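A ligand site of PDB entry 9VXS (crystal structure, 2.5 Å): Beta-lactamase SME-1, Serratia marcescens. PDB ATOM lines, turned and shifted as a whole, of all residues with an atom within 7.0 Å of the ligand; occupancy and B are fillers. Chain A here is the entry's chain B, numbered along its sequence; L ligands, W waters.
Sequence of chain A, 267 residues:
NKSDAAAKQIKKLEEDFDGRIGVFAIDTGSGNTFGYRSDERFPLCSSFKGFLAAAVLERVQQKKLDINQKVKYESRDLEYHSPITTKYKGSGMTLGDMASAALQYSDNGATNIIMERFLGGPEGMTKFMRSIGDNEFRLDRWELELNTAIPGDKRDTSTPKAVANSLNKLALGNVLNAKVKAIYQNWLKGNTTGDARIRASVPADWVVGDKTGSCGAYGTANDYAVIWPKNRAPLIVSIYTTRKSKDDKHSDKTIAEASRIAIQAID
A boron (B1) of the ligand is covalently linked to the side-chain hydroxyl (OG) of Ser 46, at 1.5 Å.
An oxygen (O2) of the ligand lies within hydrogen-bond range of the backbone carbonyl oxygen (O) of Ser 214, 3.1 Å away.
The side-chain hydroxyl (OG) of Ser 106 is in hydrogen-bond range of an oxygen (O1) of the ligand.
The backbone NH of Ser 214 is in hydrogen-bond range of an oxygen (O2) of the ligand.
N of Ser 46 is in hydrogen-bond range of O2 of the ligand, 2.5 Å away.
The side-chain amide oxygen (OD1) of Asn 108 sits close to the side-chain carboxylate (OE1) of Glu 143 (3.4 Å).
O of Ser 106 lies within hydrogen-bond range of NZ of Lys 49 (2.9 Å).
The side-chain amide nitrogen (ND2) of Asn 222 is in hydrogen-bond range of the side-chain sulfur (SG) of Cys 45 (3.8 Å).
The side-chain sulfur of Cys 45 forms a disulfide with the side-chain sulfur of Cys 215 (2.4 Å).
The side-chain amide nitrogen (ND2) of Asn 108 lies within hydrogen-bond range of the backbone carbonyl oxygen (O) of Tyr 80, 2.9 Å away.
The side-chain hydroxyl of Ser 46 is in hydrogen-bond range of the side-chain hydroxyl of Ser 106 (2.9 Å).
N of Asn 108 sits at hydrogen-bond distance from O of His 81, 3.0 Å away.
The backbone NH (N) of Asn 222 sits at hydrogen-bond distance from the backbone carbonyl oxygen (O) of Gly 213 (2.8 Å).
Merely in contact with the ligand: His 81 (3.3 Å), Asn 108 (3.5 Å), Cys 45 (3.5 Å), Asn 147 (3.6 Å), Tyr 80 (3.6 Å), Gly 213 (3.7 Å) and Leu 144 (3.8 Å).
Hydrophobic or aromatic side chains that line the ligand: Tyr 80, His 81 and Leu 144.
Within 4 Å of the ligand: Cys 45, Ser 46, Tyr 80, His 81, Ser 106, Asn 108, Leu 144, Asn 147, Gly 213 and Ser 214.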
ATOM      1  N   LEU A  44      -4.058 -13.285 -13.037  1.00  0.00           N
ATOM      2  CA  LEU A  44      -2.794 -13.892 -13.411  1.00  0.00           C
ATOM      3  C   LEU A  44      -2.921 -15.372 -13.817  1.00  0.00           C
ATOM      4  O   LEU A  44      -2.158 -15.844 -14.671  1.00  0.00           O
ATOM      5  CB  LEU A  44      -1.715 -13.722 -12.336  1.00  0.00           C
ATOM      6  CG  LEU A  44      -1.082 -12.330 -12.234  1.00  0.00           C
ATOM      7  CD1 LEU A  44      -0.465 -12.304 -10.862  1.00  0.00           C
ATOM      8  CD2 LEU A  44      -0.029 -12.034 -13.313  1.00  0.00           C
ATOM      9  N   CYS A  45      -3.789 -16.134 -13.136  1.00  0.00           N
ATOM     10  CA  CYS A  45      -3.791 -17.591 -13.292  1.00  0.00           C
ATOM     11  C   CYS A  45      -2.394 -18.166 -12.960  1.00  0.00           C
ATOM     12  O   CYS A  45      -1.685 -17.615 -12.136  1.00  0.00           O
ATOM     13  CB  CYS A  45      -4.280 -17.960 -14.686  1.00  0.00           C
ATOM     14  SG  CYS A  45      -5.781 -17.075 -15.185  1.00  0.00           S
ATOM     15  N   SER A  46      -2.005 -19.268 -13.629  1.00  0.00           N
ATOM     16  CA  SER A  46      -0.716 -19.934 -13.430  1.00  0.00           C
ATOM     17  C   SER A  46       0.463 -19.112 -13.971  1.00  0.00           C
ATOM     18  O   SER A  46       1.635 -19.488 -13.773  1.00  0.00           O
ATOM     19  CB  SER A  46      -0.677 -21.371 -13.946  1.00  0.00           C
ATOM     20  OG  SER A  46      -1.780 -22.181 -13.564  1.00  0.00           O
ATOM     21  N   SER A  47       0.189 -17.973 -14.615  1.00  0.00           N
ATOM     22  CA  SER A  47       1.224 -17.273 -15.364  1.00  0.00           C
ATOM     23  C   SER A  47       2.341 -16.761 -14.452  1.00  0.00           C
ATOM     24  O   SER A  47       3.501 -16.779 -14.858  1.00  0.00           O
ATOM     25  CB  SER A  47       0.686 -16.199 -16.296  1.00  0.00           C
ATOM     26  OG  SER A  47       0.026 -15.154 -15.593  1.00  0.00           O
ATOM     27  N   PHE A  48       2.016 -16.360 -13.211  1.00  0.00           N
ATOM     28  CA  PHE A  48       3.019 -15.892 -12.258  1.00  0.00           C
ATOM     29  C   PHE A  48       3.985 -17.036 -11.932  1.00  0.00           C
ATOM     30  O   PHE A  48       5.079 -16.813 -11.427  1.00  0.00           O
ATOM     31  CB  PHE A  48       2.353 -15.402 -10.974  1.00  0.00           C
ATOM     32  CG  PHE A  48       1.886 -16.546 -10.069  1.00  0.00           C
ATOM     33  CD1 PHE A  48       2.739 -17.096  -9.113  1.00  0.00           C
ATOM     34  CD2 PHE A  48       0.642 -17.132 -10.250  1.00  0.00           C
ATOM     35  CE1 PHE A  48       2.325 -18.182  -8.319  1.00  0.00           C
ATOM     36  CE2 PHE A  48       0.233 -18.206  -9.461  1.00  0.00           C
ATOM     37  CZ  PHE A  48       1.068 -18.723  -8.482  1.00  0.00           C
ATOM     38  N   LYS A  49       3.585 -18.273 -12.184  1.00  0.00           N
ATOM     39  CA  LYS A  49       4.454 -19.387 -11.881  1.00  0.00           C
ATOM     40  C   LYS A  49       5.768 -19.213 -12.655  1.00  0.00           C
ATOM     41  O   LYS A  49       6.797 -19.717 -12.225  1.00  0.00           O
ATOM     42  CB  LYS A  49       3.787 -20.738 -12.201  1.00  0.00           C
ATOM     43  CG  LYS A  49       2.517 -21.013 -11.432  1.00  0.00           C
ATOM     44  CD  LYS A  49       1.980 -22.390 -11.788  1.00  0.00           C
ATOM     45  CE  LYS A  49       0.812 -22.582 -10.913  1.00  0.00           C
ATOM     46  NZ  LYS A  49      -0.200 -23.497 -11.424  1.00  0.00           N
ATOM     47  N   TYR A  80      -4.747 -30.211  -6.372  1.00  0.00           N
ATOM     48  CA  TYR A  80      -5.206 -30.591  -7.701  1.00  0.00           C
ATOM     49  C   TYR A  80      -4.267 -29.995  -8.753  1.00  0.00           C
ATOM     50  O   TYR A  80      -3.842 -28.846  -8.635  1.00  0.00           O
ATOM     51  CB  TYR A  80      -6.674 -30.174  -7.893  1.00  0.00           C
ATOM     52  CG  TYR A  80      -7.196 -30.516  -9.291  1.00  0.00           C
ATOM     53  CD1 TYR A  80      -7.503 -31.833  -9.630  1.00  0.00           C
ATOM     54  CD2 TYR A  80      -7.351 -29.535 -10.272  1.00  0.00           C
ATOM     55  CE1 TYR A  80      -7.941 -32.167 -10.901  1.00  0.00           C
ATOM     56  CE2 TYR A  80      -7.804 -29.852 -11.539  1.00  0.00           C
ATOM     57  CZ  TYR A  80      -8.089 -31.172 -11.843  1.00  0.00           C
ATOM     58  OH  TYR A  80      -8.516 -31.533 -13.069  1.00  0.00           O
ATOM     59  N   HIS A  81      -3.930 -30.805  -9.764  1.00  0.00           N
ATOM     60  CA  HIS A  81      -3.051 -30.503 -10.899  1.00  0.00           C
ATOM     61  C   HIS A  81      -1.591 -30.384 -10.451  1.00  0.00           C
ATOM     62  O   HIS A  81      -0.956 -29.335 -10.622  1.00  0.00           O
ATOM     63  CB  HIS A  81      -3.622 -29.430 -11.848  1.00  0.00           C
ATOM     64  CG  HIS A  81      -2.851 -29.353 -13.132  1.00  0.00           C
ATOM     65  ND1 HIS A  81      -3.042 -30.232 -14.176  1.00  0.00           N
ATOM     66  CD2 HIS A  81      -1.828 -28.554 -13.519  1.00  0.00           C
ATOM     67  CE1 HIS A  81      -2.203 -29.961 -15.166  1.00  0.00           C
ATOM     68  NE2 HIS A  81      -1.444 -28.941 -14.790  1.00  0.00           N
ATOM     69  N   SER A  82      -1.087 -31.510  -9.911  1.00  0.00           N
ATOM     70  CA  SER A  82       0.285 -31.684  -9.450  1.00  0.00           C
ATOM     71  C   SER A  82       0.899 -32.894 -10.144  1.00  0.00           C
ATOM     72  O   SER A  82       1.311 -33.882  -9.535  1.00  0.00           O
ATOM     73  CB  SER A  82       0.353 -31.790  -7.943  1.00  0.00           C
ATOM     74  OG  SER A  82      -0.057 -30.580  -7.306  1.00  0.00           O
ATOM     75  N   TYR A 105       4.953 -27.500 -16.247  1.00  0.00           N
ATOM     76  CA  TYR A 105       3.719 -28.262 -16.206  1.00  0.00           C
ATOM     77  C   TYR A 105       2.712 -27.543 -15.324  1.00  0.00           C
ATOM     78  O   TYR A 105       1.701 -28.130 -14.963  1.00  0.00           O
ATOM     79  CB  TYR A 105       3.941 -29.698 -15.713  1.00  0.00           C
ATOM     80  CG  TYR A 105       4.862 -30.490 -16.617  1.00  0.00           C
ATOM     81  CD1 TYR A 105       6.256 -30.456 -16.469  1.00  0.00           C
ATOM     82  CD2 TYR A 105       4.329 -31.256 -17.641  1.00  0.00           C
ATOM     83  CE1 TYR A 105       7.092 -31.171 -17.309  1.00  0.00           C
ATOM     84  CE2 TYR A 105       5.158 -31.988 -18.489  1.00  0.00           C
ATOM     85  CZ  TYR A 105       6.523 -31.946 -18.309  1.00  0.00           C
ATOM     86  OH  TYR A 105       7.235 -32.670 -19.193  1.00  0.00           O
ATOM     87  N   SER A 106       3.045 -26.298 -14.936  1.00  0.00           N
ATOM     88  CA  SER A 106       2.101 -25.469 -14.206  1.00  0.00           C
ATOM     89  C   SER A 106       1.687 -26.176 -12.903  1.00  0.00           C
ATOM     90  O   SER A 106       0.530 -26.076 -12.449  1.00  0.00           O
ATOM     91  CB  SER A 106       0.912 -25.161 -15.110  1.00  0.00           C
ATOM     92  OG  SER A 106       0.164 -24.076 -14.602  1.00  0.00           O
ATOM     93  N   ASP A 107       2.647 -26.862 -12.267  1.00  0.00           N
ATOM     94  CA  ASP A 107       2.399 -27.780 -11.164  1.00  0.00           C
ATOM     95  C   ASP A 107       2.013 -27.005  -9.899  1.00  0.00           C
ATOM     96  O   ASP A 107       2.846 -26.262  -9.370  1.00  0.00           O
ATOM     97  CB  ASP A 107       3.579 -28.712 -10.966  1.00  0.00           C
ATOM     98  CG  ASP A 107       3.397 -29.854  -9.974  1.00  0.00           C
ATOM     99  OD1 ASP A 107       3.153 -29.569  -8.761  1.00  0.00           O
ATOM    100  OD2 ASP A 107       3.548 -31.024 -10.422  1.00  0.00           O
ATOM    101  N   ASN A 108       0.802 -27.249  -9.384  1.00  0.00           N
ATOM    102  CA  ASN A 108       0.302 -26.531  -8.217  1.00  0.00           C
ATOM    103  C   ASN A 108       1.023 -26.903  -6.904  1.00  0.00           C
ATOM    104  O   ASN A 108       1.319 -26.041  -6.084  1.00  0.00           O
ATOM    105  CB  ASN A 108      -1.223 -26.614  -8.108  1.00  0.00           C
ATOM    106  CG  ASN A 108      -1.936 -25.772  -9.146  1.00  0.00           C
ATOM    107  OD1 ASN A 108      -1.525 -24.628  -9.408  1.00  0.00           O
ATOM    108  ND2 ASN A 108      -2.996 -26.326  -9.737  1.00  0.00           N
ATOM    109  N   GLU A 143      -2.621 -21.242  -4.510  1.00  0.00           N
ATOM    110  CA  GLU A 143      -3.333 -22.162  -5.386  1.00  0.00           C
ATOM    111  C   GLU A 143      -4.304 -22.953  -4.513  1.00  0.00           C
ATOM    112  O   GLU A 143      -3.890 -23.367  -3.452  1.00  0.00           O
ATOM    113  CB  GLU A 143      -2.274 -23.060  -6.030  1.00  0.00           C
ATOM    114  CG  GLU A 143      -1.440 -22.374  -7.124  1.00  0.00           C
ATOM    115  CD  GLU A 143      -2.239 -21.859  -8.319  1.00  0.00           C
ATOM    116  OE1 GLU A 143      -1.622 -21.242  -9.212  1.00  0.00           O
ATOM    117  OE2 GLU A 143      -3.482 -22.035  -8.363  1.00  0.00           O
ATOM    118  N   LEU A 144      -5.554 -23.192  -4.949  1.00  0.00           N
ATOM    119  CA  LEU A 144      -6.088 -22.916  -6.276  1.00  0.00           C
ATOM    120  C   LEU A 144      -7.010 -21.696  -6.220  1.00  0.00           C
ATOM    121  O   LEU A 144      -7.503 -21.239  -7.251  1.00  0.00           O
ATOM    122  CB  LEU A 144      -6.834 -24.095  -6.918  1.00  0.00           C
ATOM    123  CG  LEU A 144      -6.013 -25.169  -7.653  1.00  0.00           C
ATOM    124  CD1 LEU A 144      -5.340 -26.149  -6.737  1.00  0.00           C
ATOM    125  CD2 LEU A 144      -6.922 -25.904  -8.632  1.00  0.00           C
ATOM    126  N   LEU A 146      -6.657 -18.717  -5.981  1.00  0.00           N
ATOM    127  CA  LEU A 146      -6.237 -17.493  -6.647  1.00  0.00           C
ATOM    128  C   LEU A 146      -6.801 -17.416  -8.055  1.00  0.00           C
ATOM    129  O   LEU A 146      -6.630 -16.400  -8.740  1.00  0.00           O
ATOM    130  CB  LEU A 146      -4.709 -17.331  -6.677  1.00  0.00           C
ATOM    131  CG  LEU A 146      -3.888 -18.437  -7.349  1.00  0.00           C
ATOM    132  CD1 LEU A 146      -4.064 -18.510  -8.885  1.00  0.00           C
ATOM    133  CD2 LEU A 146      -2.421 -18.270  -6.955  1.00  0.00           C
ATOM    134  N   ASN A 147      -7.459 -18.500  -8.509  1.00  0.00           N
ATOM    135  CA  ASN A 147      -7.848 -18.601  -9.903  1.00  0.00           C
ATOM    136  C   ASN A 147      -9.317 -18.213 -10.086  1.00  0.00           C
ATOM    137  O   ASN A 147      -9.869 -18.498 -11.144  1.00  0.00           O
ATOM    138  CB  ASN A 147      -7.676 -20.029 -10.428  1.00  0.00           C
ATOM    139  CG  ASN A 147      -6.247 -20.517 -10.538  1.00  0.00           C
ATOM    140  OD1 ASN A 147      -5.547 -20.192 -11.492  1.00  0.00           O
ATOM    141  ND2 ASN A 147      -5.830 -21.361  -9.600  1.00  0.00           N
ATOM    142  N   THR A 193       2.789 -26.293 -22.097  1.00  0.00           N
ATOM    143  CA  THR A 193       1.351 -26.084 -22.023  1.00  0.00           C
ATOM    144  C   THR A 193       0.896 -25.063 -23.065  1.00  0.00           C
ATOM    145  O   THR A 193      -0.297 -24.751 -23.118  1.00  0.00           O
ATOM    146  CB  THR A 193       0.894 -25.648 -20.620  1.00  0.00           C
ATOM    147  OG1 THR A 193       1.532 -24.419 -20.270  1.00  0.00           O
ATOM    148  CG2 THR A 193       1.112 -26.716 -19.569  1.00  0.00           C
ATOM    149  N   LYS A 211       5.037 -18.851 -20.689  1.00  0.00           N
ATOM    150  CA  LYS A 211       4.271 -19.499 -19.634  1.00  0.00           C
ATOM    151  C   LYS A 211       2.798 -19.144 -19.843  1.00  0.00           C
ATOM    152  O   LYS A 211       2.476 -17.996 -20.059  1.00  0.00           O
ATOM    153  CB  LYS A 211       4.718 -19.049 -18.244  1.00  0.00           C
ATOM    154  CG  LYS A 211       3.902 -19.594 -17.062  1.00  0.00           C
ATOM    155  CD  LYS A 211       4.083 -21.102 -16.916  1.00  0.00           C
ATOM    156  CE  LYS A 211       3.299 -21.745 -15.828  1.00  0.00           C
ATOM    157  NZ  LYS A 211       2.025 -22.272 -16.340  1.00  0.00           N
ATOM    158  N   THR A 212       1.927 -20.156 -19.758  1.00  0.00           N
ATOM    159  CA  THR A 212       0.512 -19.923 -19.990  1.00  0.00           C
ATOM    160  C   THR A 212      -0.189 -19.756 -18.654  1.00  0.00           C
ATOM    161  O   THR A 212       0.382 -20.128 -17.618  1.00  0.00           O
ATOM    162  CB  THR A 212      -0.054 -21.126 -20.737  1.00  0.00           C
ATOM    163  OG1 THR A 212       0.076 -22.216 -19.829  1.00  0.00           O
ATOM    164  CG2 THR A 212       0.728 -21.445 -21.983  1.00  0.00           C
ATOM    165  N   GLY A 213      -1.429 -19.244 -18.682  1.00  0.00           N
ATOM    166  CA  GLY A 213      -2.317 -19.384 -17.531  1.00  0.00           C
ATOM    167  C   GLY A 213      -3.759 -19.669 -17.973  1.00  0.00           C
ATOM    168  O   GLY A 213      -4.217 -19.129 -18.985  1.00  0.00           O
ATOM    169  N   SER A 214      -4.468 -20.499 -17.199  1.00  0.00           N
ATOM    170  CA  SER A 214      -5.884 -20.792 -17.409  1.00  0.00           C
ATOM    171  C   SER A 214      -6.599 -20.895 -16.073  1.00  0.00           C
ATOM    172  O   SER A 214      -6.182 -21.654 -15.186  1.00  0.00           O
ATOM    173  CB  SER A 214      -6.054 -22.054 -18.233  1.00  0.00           C
ATOM    174  OG  SER A 214      -5.186 -22.042 -19.354  1.00  0.00           O
ATOM    175  N   CYS A 215      -7.664 -20.106 -15.897  1.00  0.00           N
ATOM    176  CA  CYS A 215      -8.278 -19.961 -14.592  1.00  0.00           C
ATOM    177  C   CYS A 215      -9.371 -20.998 -14.363  1.00  0.00           C
ATOM    178  O   CYS A 215      -9.606 -21.417 -13.238  1.00  0.00           O
ATOM    179  CB  CYS A 215      -8.774 -18.538 -14.349  1.00  0.00           C
ATOM    180  SG  CYS A 215      -7.526 -17.465 -13.568  1.00  0.00           S
ATOM    181  N   GLY A 216     -10.027 -21.429 -15.446  1.00  0.00           N
ATOM    182  CA  GLY A 216     -11.187 -22.306 -15.312  1.00  0.00           C
ATOM    183  C   GLY A 216     -12.462 -21.572 -14.872  1.00  0.00           C
ATOM    184  O   GLY A 216     -13.447 -22.204 -14.493  1.00  0.00           O
ATOM    185  N   ASN A 222      -4.310 -16.805 -20.491  1.00  0.00           N
ATOM    186  CA  ASN A 222      -3.308 -15.843 -20.920  1.00  0.00           C
ATOM    187  C   ASN A 222      -2.064 -16.595 -21.394  1.00  0.00           C
ATOM    188  O   ASN A 222      -1.977 -17.807 -21.253  1.00  0.00           O
ATOM    189  CB  ASN A 222      -2.981 -14.849 -19.816  1.00  0.00           C
ATOM    190  CG  ASN A 222      -2.728 -15.542 -18.494  1.00  0.00           C
ATOM    191  OD1 ASN A 222      -1.935 -16.482 -18.447  1.00  0.00           O
ATOM    192  ND2 ASN A 222      -3.410 -15.153 -17.423  1.00  0.00           N
HETATM  193  B1  LIG L   1      -2.953 -22.627 -14.367  1.00  0.00           B
HETATM  194  C1  LIG L   1      -3.763 -23.605 -13.475  1.00  0.00           C
HETATM  195  C2  LIG L   1      -3.666 -24.837 -14.135  1.00  0.00           C
HETATM  196  C3  LIG L   1      -2.778 -24.719 -15.339  1.00  0.00           C
HETATM  197  C4  LIG L   1      -4.352 -25.953 -13.693  1.00  0.00           C
HETATM  198  C5  LIG L   1      -5.110 -25.803 -12.561  1.00  0.00           C
HETATM  199  C6  LIG L   1      -5.239 -24.624 -11.863  1.00  0.00           C
HETATM  200  C7  LIG L   1      -4.545 -23.517 -12.319  1.00  0.00           C
HETATM  201  F1  LIG L   1      -5.767 -26.902 -12.106  1.00  0.00           F
HETATM  202  O1  LIG L   1      -2.260 -23.365 -15.326  1.00  0.00           O
HETATM  203  O2  LIG L   1      -3.154 -21.302 -14.421  1.00  0.00           O
HETATM  204  O   HOH W   1      -2.940 -20.841 -11.285  1.00  0.00           O
